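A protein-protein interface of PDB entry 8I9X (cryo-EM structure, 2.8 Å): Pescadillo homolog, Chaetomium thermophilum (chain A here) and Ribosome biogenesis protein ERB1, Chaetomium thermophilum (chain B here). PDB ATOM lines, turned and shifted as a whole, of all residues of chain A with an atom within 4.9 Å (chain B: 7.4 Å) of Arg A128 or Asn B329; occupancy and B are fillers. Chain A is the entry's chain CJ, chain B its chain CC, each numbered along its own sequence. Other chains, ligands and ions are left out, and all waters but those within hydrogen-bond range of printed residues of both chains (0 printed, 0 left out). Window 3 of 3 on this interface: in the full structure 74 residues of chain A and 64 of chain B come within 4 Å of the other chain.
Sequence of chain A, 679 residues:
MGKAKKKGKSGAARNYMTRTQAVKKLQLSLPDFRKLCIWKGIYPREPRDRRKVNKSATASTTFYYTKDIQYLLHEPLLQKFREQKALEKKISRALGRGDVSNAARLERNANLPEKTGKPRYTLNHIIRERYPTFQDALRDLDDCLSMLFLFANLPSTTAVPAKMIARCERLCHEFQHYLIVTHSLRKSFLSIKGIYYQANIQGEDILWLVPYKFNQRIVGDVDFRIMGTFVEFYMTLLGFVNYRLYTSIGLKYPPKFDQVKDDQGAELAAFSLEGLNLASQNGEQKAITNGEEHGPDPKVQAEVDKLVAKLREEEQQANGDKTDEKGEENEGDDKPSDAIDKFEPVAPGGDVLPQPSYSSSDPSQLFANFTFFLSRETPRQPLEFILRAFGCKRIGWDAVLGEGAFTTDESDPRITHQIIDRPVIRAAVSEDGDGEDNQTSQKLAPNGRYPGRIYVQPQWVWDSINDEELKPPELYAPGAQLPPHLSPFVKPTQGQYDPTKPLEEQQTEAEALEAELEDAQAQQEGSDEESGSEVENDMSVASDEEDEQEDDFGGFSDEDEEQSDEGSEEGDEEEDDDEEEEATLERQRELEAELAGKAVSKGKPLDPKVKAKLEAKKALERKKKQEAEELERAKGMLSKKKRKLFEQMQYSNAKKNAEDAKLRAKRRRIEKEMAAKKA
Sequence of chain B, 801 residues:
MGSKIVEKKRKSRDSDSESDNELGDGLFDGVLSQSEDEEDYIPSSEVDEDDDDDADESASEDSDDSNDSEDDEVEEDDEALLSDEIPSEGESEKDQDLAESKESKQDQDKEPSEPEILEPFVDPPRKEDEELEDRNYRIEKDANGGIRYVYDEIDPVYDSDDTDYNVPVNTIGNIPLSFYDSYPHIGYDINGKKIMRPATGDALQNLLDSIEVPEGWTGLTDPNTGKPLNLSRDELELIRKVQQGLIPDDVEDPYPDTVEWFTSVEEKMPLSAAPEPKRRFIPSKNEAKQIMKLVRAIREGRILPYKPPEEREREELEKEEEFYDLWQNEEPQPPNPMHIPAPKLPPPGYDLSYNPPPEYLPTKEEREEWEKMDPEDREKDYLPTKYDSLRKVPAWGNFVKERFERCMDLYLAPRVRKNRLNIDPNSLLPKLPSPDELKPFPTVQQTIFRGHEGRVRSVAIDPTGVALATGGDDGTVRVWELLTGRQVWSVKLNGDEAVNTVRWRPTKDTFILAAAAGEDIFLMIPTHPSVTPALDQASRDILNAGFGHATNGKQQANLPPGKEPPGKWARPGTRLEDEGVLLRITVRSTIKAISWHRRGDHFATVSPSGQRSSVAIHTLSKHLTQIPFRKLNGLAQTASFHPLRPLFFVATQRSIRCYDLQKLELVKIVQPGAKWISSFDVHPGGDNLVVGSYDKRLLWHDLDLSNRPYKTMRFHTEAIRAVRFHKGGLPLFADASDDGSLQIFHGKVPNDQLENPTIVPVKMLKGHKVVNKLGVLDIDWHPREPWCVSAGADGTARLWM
The side-chain carboxylate of Asp B325 lies within hydrogen-bond range of the backbone NH of Trp B327, 2.6 Å away.
The guanidinium group of Arg A128 is in hydrogen-bond range of the backbone carbonyl oxygen of Asn B329 (3.4 Å).
O of Tyr A131 sits at hydrogen-bond distance from NE1 of Trp B327, 3.1 Å away.
Of the printed residues of chain B, Ile A127 touches Leu B326.
Of chain B, only Leu B326 (3.8 Å) and Asn B329 (3.4 Å) come within 4 Å of Arg A128.
Printed residues of chain B within 4 Å of Tyr A131: Trp B327 (3.1 Å).
Printed residues of chain B within 4 Å of Pro A132: Trp B327, Glu B330 and Gln B333.
Tyr B324 touches none of the printed residues of chain A.
Of chain A, only Arg A128 (3.4 Å) comes within 4 Å of Asn B329.
Of the printed residues of chain A, Glu B330 touches Pro A132.
Printed residues of chain A within 4 Å of Gln B333: Pro A132 (3.3 Å).
The nearest printed residue of chain A that does not touch Leu B326 is His A125 (5.4 Å).
Hydrophobic or aromatic side chains of chain B within 4 Å of the printed part of chain A: Leu B326 and Trp B327.
Among the printed residues, 8 pairs touch across the chains.
Among the printed residues, merely in contact across the chains: Asn A124 with Leu B326, Ile A127 with Leu B326, Arg A128 with Leu B326, Pro A132 with Trp B327, Pro A132 with Glu B330 and Pro A132 with Gln B333.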
ATOM      1  N   ASN A 124     -26.953   2.387 -11.356  1.00  0.00           N
ATOM      2  CA  ASN A 124     -27.338   1.031 -10.985  1.00  0.00           C
ATOM      3  C   ASN A 124     -27.880   0.240 -12.167  1.00  0.00           C
ATOM      4  O   ASN A 124     -27.449  -0.893 -12.403  1.00  0.00           O
ATOM      5  CB  ASN A 124     -28.389   1.068  -9.873  1.00  0.00           C
ATOM      6  CG  ASN A 124     -27.939   1.870  -8.673  1.00  0.00           C
ATOM      7  OD1 ASN A 124     -26.757   1.894  -8.337  1.00  0.00           O
ATOM      8  ND2 ASN A 124     -28.884   2.523  -8.013  1.00  0.00           N
ATOM      9  N   HIS A 125     -28.820   0.821 -12.912  1.00  0.00           N
ATOM     10  CA  HIS A 125     -29.365   0.138 -14.077  1.00  0.00           C
ATOM     11  C   HIS A 125     -28.312  -0.056 -15.159  1.00  0.00           C
ATOM     12  O   HIS A 125     -28.328  -1.077 -15.854  1.00  0.00           O
ATOM     13  CB  HIS A 125     -30.570   0.903 -14.621  1.00  0.00           C
ATOM     14  CG  HIS A 125     -30.303   2.352 -14.881  1.00  0.00           C
ATOM     15  ND1 HIS A 125     -30.383   3.310 -13.893  1.00  0.00           N
ATOM     16  CD2 HIS A 125     -29.972   3.011 -16.016  1.00  0.00           C
ATOM     17  CE1 HIS A 125     -30.104   4.494 -14.407  1.00  0.00           C
ATOM     18  NE2 HIS A 125     -29.852   4.341 -15.694  1.00  0.00           N
ATOM     19  N   ILE A 126     -27.391   0.898 -15.313  1.00  0.00           N
ATOM     20  CA  ILE A 126     -26.314   0.717 -16.280  1.00  0.00           C
ATOM     21  C   ILE A 126     -25.449  -0.474 -15.904  1.00  0.00           C
ATOM     22  O   ILE A 126     -25.110  -1.301 -16.758  1.00  0.00           O
ATOM     23  CB  ILE A 126     -25.473   1.997 -16.412  1.00  0.00           C
ATOM     24  CG1 ILE A 126     -26.267   3.100 -17.088  1.00  0.00           C
ATOM     25  CG2 ILE A 126     -24.204   1.732 -17.180  1.00  0.00           C
ATOM     26  CD1 ILE A 126     -25.506   4.360 -17.123  1.00  0.00           C
ATOM     27  N   ILE A 127     -25.074  -0.585 -14.628  1.00  0.00           N
ATOM     28  CA  ILE A 127     -24.262  -1.726 -14.223  1.00  0.00           C
ATOM     29  C   ILE A 127     -25.037  -3.021 -14.416  1.00  0.00           C
ATOM     30  O   ILE A 127     -24.490  -4.015 -14.909  1.00  0.00           O
ATOM     31  CB  ILE A 127     -23.788  -1.557 -12.770  1.00  0.00           C
ATOM     32  CG1 ILE A 127     -22.677  -0.515 -12.703  1.00  0.00           C
ATOM     33  CG2 ILE A 127     -23.259  -2.872 -12.225  1.00  0.00           C
ATOM     34  CD1 ILE A 127     -22.383  -0.041 -11.314  1.00  0.00           C
ATOM     35  N   ARG A 128     -26.324  -3.024 -14.060  1.00  0.00           N
ATOM     36  CA  ARG A 128     -27.155  -4.214 -14.205  1.00  0.00           C
ATOM     37  C   ARG A 128     -27.262  -4.665 -15.654  1.00  0.00           C
ATOM     38  O   ARG A 128     -27.214  -5.870 -15.925  1.00  0.00           O
ATOM     39  CB  ARG A 128     -28.545  -3.941 -13.631  1.00  0.00           C
ATOM     40  CG  ARG A 128     -29.540  -5.088 -13.729  1.00  0.00           C
ATOM     41  CD  ARG A 128     -29.127  -6.278 -12.882  1.00  0.00           C
ATOM     42  NE  ARG A 128     -30.104  -7.360 -12.950  1.00  0.00           N
ATOM     43  CZ  ARG A 128     -30.120  -8.304 -13.880  1.00  0.00           C
ATOM     44  NH1 ARG A 128     -29.224  -8.332 -14.853  1.00  0.00           N
ATOM     45  NH2 ARG A 128     -31.059  -9.244 -13.834  1.00  0.00           N
ATOM     46  N   GLU A 129     -27.408  -3.730 -16.595  1.00  0.00           N
ATOM     47  CA  GLU A 129     -27.539  -4.119 -17.995  1.00  0.00           C
ATOM     48  C   GLU A 129     -26.190  -4.465 -18.619  1.00  0.00           C
ATOM     49  O   GLU A 129     -26.119  -5.339 -19.490  1.00  0.00           O
ATOM     50  CB  GLU A 129     -28.249  -3.020 -18.792  1.00  0.00           C
ATOM     51  CG  GLU A 129     -27.553  -1.671 -18.837  1.00  0.00           C
ATOM     52  CD  GLU A 129     -26.525  -1.575 -19.946  1.00  0.00           C
ATOM     53  OE1 GLU A 129     -26.598  -2.380 -20.898  1.00  0.00           O
ATOM     54  OE2 GLU A 129     -25.653  -0.685 -19.873  1.00  0.00           O
ATOM     55  N   ARG A 130     -25.113  -3.797 -18.200  1.00  0.00           N
ATOM     56  CA  ARG A 130     -23.792  -4.133 -18.721  1.00  0.00           C
ATOM     57  C   ARG A 130     -23.359  -5.517 -18.270  1.00  0.00           C
ATOM     58  O   ARG A 130     -22.860  -6.315 -19.071  1.00  0.00           O
ATOM     59  CB  ARG A 130     -22.761  -3.094 -18.287  1.00  0.00           C
ATOM     60  CG  ARG A 130     -22.809  -1.808 -19.065  1.00  0.00           C
ATOM     61  CD  ARG A 130     -21.521  -1.045 -18.880  1.00  0.00           C
ATOM     62  NE  ARG A 130     -20.399  -1.724 -19.512  1.00  0.00           N
ATOM     63  CZ  ARG A 130     -19.150  -1.281 -19.494  1.00  0.00           C
ATOM     64  NH1 ARG A 130     -18.827  -0.151 -18.889  1.00  0.00           N
ATOM     65  NH2 ARG A 130     -18.203  -1.988 -20.102  1.00  0.00           N
ATOM     66  N   TYR A 131     -23.539  -5.822 -16.988  1.00  0.00           N
ATOM     67  CA  TYR A 131     -23.197  -7.131 -16.447  1.00  0.00           C
ATOM     68  C   TYR A 131     -24.473  -7.760 -15.915  1.00  0.00           C
ATOM     69  O   TYR A 131     -24.820  -7.578 -14.739  1.00  0.00           O
ATOM     70  CB  TYR A 131     -22.145  -7.018 -15.343  1.00  0.00           C
ATOM     71  CG  TYR A 131     -21.055  -6.018 -15.634  1.00  0.00           C
ATOM     72  CD1 TYR A 131     -20.302  -6.105 -16.792  1.00  0.00           C
ATOM     73  CD2 TYR A 131     -20.775  -4.992 -14.745  1.00  0.00           C
ATOM     74  CE1 TYR A 131     -19.306  -5.197 -17.061  1.00  0.00           C
ATOM     75  CE2 TYR A 131     -19.778  -4.078 -15.006  1.00  0.00           C
ATOM     76  CZ  TYR A 131     -19.044  -4.186 -16.164  1.00  0.00           C
ATOM     77  OH  TYR A 131     -18.048  -3.275 -16.429  1.00  0.00           O
ATOM     78  N   PRO A 132     -25.211  -8.510 -16.736  1.00  0.00           N
ATOM     79  CA  PRO A 132     -26.378  -9.228 -16.215  1.00  0.00           C
ATOM     80  C   PRO A 132     -26.010 -10.364 -15.286  1.00  0.00           C
ATOM     81  O   PRO A 132     -26.911 -10.989 -14.713  1.00  0.00           O
ATOM     82  CB  PRO A 132     -27.064  -9.743 -17.486  1.00  0.00           C
ATOM     83  CG  PRO A 132     -25.954  -9.882 -18.465  1.00  0.00           C
ATOM     84  CD  PRO A 132     -25.012  -8.745 -18.176  1.00  0.00           C
ATOM     85  N   TYR B 324     -28.268  -2.525  -1.352  1.00  0.00           N
ATOM     86  CA  TYR B 324     -29.099  -3.664  -1.709  1.00  0.00           C
ATOM     87  C   TYR B 324     -28.384  -4.483  -2.771  1.00  0.00           C
ATOM     88  O   TYR B 324     -27.436  -4.019  -3.408  1.00  0.00           O
ATOM     89  CB  TYR B 324     -30.482  -3.218  -2.197  1.00  0.00           C
ATOM     90  CG  TYR B 324     -30.512  -2.714  -3.621  1.00  0.00           C
ATOM     91  CD1 TYR B 324     -30.130  -1.417  -3.925  1.00  0.00           C
ATOM     92  CD2 TYR B 324     -30.943  -3.528  -4.659  1.00  0.00           C
ATOM     93  CE1 TYR B 324     -30.161  -0.949  -5.223  1.00  0.00           C
ATOM     94  CE2 TYR B 324     -30.977  -3.070  -5.958  1.00  0.00           C
ATOM     95  CZ  TYR B 324     -30.585  -1.780  -6.235  1.00  0.00           C
ATOM     96  OH  TYR B 324     -30.620  -1.319  -7.530  1.00  0.00           O
ATOM     97  N   ASP B 325     -28.849  -5.716  -2.953  1.00  0.00           N
ATOM     98  CA  ASP B 325     -28.222  -6.637  -3.891  1.00  0.00           C
ATOM     99  C   ASP B 325     -28.725  -6.305  -5.291  1.00  0.00           C
ATOM    100  O   ASP B 325     -29.930  -6.371  -5.554  1.00  0.00           O
ATOM    101  CB  ASP B 325     -28.545  -8.081  -3.497  1.00  0.00           C
ATOM    102  CG  ASP B 325     -28.190  -9.108  -4.576  1.00  0.00           C
ATOM    103  OD1 ASP B 325     -27.649  -8.756  -5.646  1.00  0.00           O
ATOM    104  OD2 ASP B 325     -28.463 -10.304  -4.341  1.00  0.00           O
ATOM    105  N   LEU B 326     -27.801  -5.948  -6.184  1.00  0.00           N
ATOM    106  CA  LEU B 326     -28.187  -5.620  -7.551  1.00  0.00           C
ATOM    107  C   LEU B 326     -28.796  -6.821  -8.257  1.00  0.00           C
ATOM    108  O   LEU B 326     -29.800  -6.689  -8.967  1.00  0.00           O
ATOM    109  CB  LEU B 326     -26.981  -5.103  -8.330  1.00  0.00           C
ATOM    110  CG  LEU B 326     -27.312  -4.279  -9.571  1.00  0.00           C
ATOM    111  CD1 LEU B 326     -28.052  -3.008  -9.190  1.00  0.00           C
ATOM    112  CD2 LEU B 326     -26.051  -3.959 -10.339  1.00  0.00           C
ATOM    113  N   TRP B 327     -28.205  -7.996  -8.082  1.00  0.00           N
ATOM    114  CA  TRP B 327     -28.702  -9.219  -8.708  1.00  0.00           C
ATOM    115  C   TRP B 327     -29.646  -9.971  -7.778  1.00  0.00           C
ATOM    116  O   TRP B 327     -29.481 -11.166  -7.535  1.00  0.00           O
ATOM    117  CB  TRP B 327     -27.535 -10.102  -9.129  1.00  0.00           C
ATOM    118  CG  TRP B 327     -26.596  -9.435 -10.082  1.00  0.00           C
ATOM    119  CD1 TRP B 327     -26.574  -9.568 -11.439  1.00  0.00           C
ATOM    120  CD2 TRP B 327     -25.516  -8.556  -9.748  1.00  0.00           C
ATOM    121  NE1 TRP B 327     -25.560  -8.810 -11.972  1.00  0.00           N
ATOM    122  CE2 TRP B 327     -24.895  -8.181 -10.954  1.00  0.00           C
ATOM    123  CE3 TRP B 327     -25.019  -8.044  -8.548  1.00  0.00           C
ATOM    124  CZ2 TRP B 327     -23.804  -7.319 -10.994  1.00  0.00           C
ATOM    125  CZ3 TRP B 327     -23.936  -7.186  -8.591  1.00  0.00           C
ATOM    126  CH2 TRP B 327     -23.341  -6.833  -9.804  1.00  0.00           C
ATOM    127  N   GLN B 328     -30.650  -9.273  -7.242  1.00  0.00           N
ATOM    128  CA  GLN B 328     -31.616  -9.925  -6.362  1.00  0.00           C
ATOM    129  C   GLN B 328     -32.411 -10.982  -7.116  1.00  0.00           C
ATOM    130  O   GLN B 328     -32.645 -12.083  -6.604  1.00  0.00           O
ATOM    131  CB  GLN B 328     -32.549  -8.882  -5.745  1.00  0.00           C
ATOM    132  CG  GLN B 328     -33.619  -9.466  -4.834  1.00  0.00           C
ATOM    133  CD  GLN B 328     -33.052  -9.994  -3.531  1.00  0.00           C
ATOM    134  OE1 GLN B 328     -32.180  -9.373  -2.922  1.00  0.00           O
ATOM    135  NE2 GLN B 328     -33.547 -11.147  -3.094  1.00  0.00           N
ATOM    136  N   ASN B 329     -32.830 -10.664  -8.336  1.00  0.00           N
ATOM    137  CA  ASN B 329     -33.491 -11.608  -9.232  1.00  0.00           C
ATOM    138  C   ASN B 329     -32.581 -11.756 -10.448  1.00  0.00           C
ATOM    139  O   ASN B 329     -32.721 -11.039 -11.440  1.00  0.00           O
ATOM    140  CB  ASN B 329     -34.886 -11.126  -9.618  1.00  0.00           C
ATOM    141  CG  ASN B 329     -35.834 -11.080  -8.435  1.00  0.00           C
ATOM    142  OD1 ASN B 329     -35.527 -10.487  -7.401  1.00  0.00           O
ATOM    143  ND2 ASN B 329     -36.996 -11.707  -8.583  1.00  0.00           N
ATOM    144  N   GLU B 330     -31.643 -12.693 -10.361  1.00  0.00           N
ATOM    145  CA  GLU B 330     -30.619 -12.888 -11.378  1.00  0.00           C
ATOM    146  C   GLU B 330     -30.915 -14.151 -12.172  1.00  0.00           C
ATOM    147  O   GLU B 330     -31.096 -15.227 -11.593  1.00  0.00           O
ATOM    148  CB  GLU B 330     -29.232 -12.978 -10.740  1.00  0.00           C
ATOM    149  CG  GLU B 330     -28.114 -13.295 -11.713  1.00  0.00           C
ATOM    150  CD  GLU B 330     -26.781 -13.483 -11.018  1.00  0.00           C
ATOM    151  OE1 GLU B 330     -26.613 -14.505 -10.321  1.00  0.00           O
ATOM    152  OE2 GLU B 330     -25.901 -12.610 -11.169  1.00  0.00           O
ATOM    153  N   GLU B 331     -30.960 -14.016 -13.492  1.00  0.00           N
ATOM    154  CA  GLU B 331     -31.188 -15.130 -14.396  1.00  0.00           C
ATOM    155  C   GLU B 331     -30.202 -15.062 -15.550  1.00  0.00           C
ATOM    156  O   GLU B 331     -29.878 -13.972 -16.033  1.00  0.00           O
ATOM    157  CB  GLU B 331     -32.622 -15.121 -14.948  1.00  0.00           C
ATOM    158  CG  GLU B 331     -33.705 -14.982 -13.889  1.00  0.00           C
ATOM    159  CD  GLU B 331     -35.039 -15.540 -14.342  1.00  0.00           C
ATOM    160  OE1 GLU B 331     -35.150 -15.940 -15.520  1.00  0.00           O
ATOM    161  OE2 GLU B 331     -35.979 -15.581 -13.520  1.00  0.00           O
ATOM    162  N   GLN B 333     -28.685 -14.984 -19.223  1.00  0.00           N
ATOM    163  CA  GLN B 333     -29.194 -14.363 -20.433  1.00  0.00           C
ATOM    164  C   GLN B 333     -28.344 -14.770 -21.626  1.00  0.00           C
ATOM    165  O   GLN B 333     -27.141 -15.008 -21.483  1.00  0.00           O
ATOM    166  CB  GLN B 333     -29.206 -12.833 -20.305  1.00  0.00           C
ATOM    167  CG  GLN B 333     -30.188 -12.308 -19.270  1.00  0.00           C
ATOM    168  CD  GLN B 333     -30.176 -10.796 -19.166  1.00  0.00           C
ATOM    169  OE1 GLN B 333     -29.392 -10.122 -19.833  1.00  0.00           O
ATOM    170  NE2 GLN B 333     -31.049 -10.254 -18.324  1.00  0.00           N
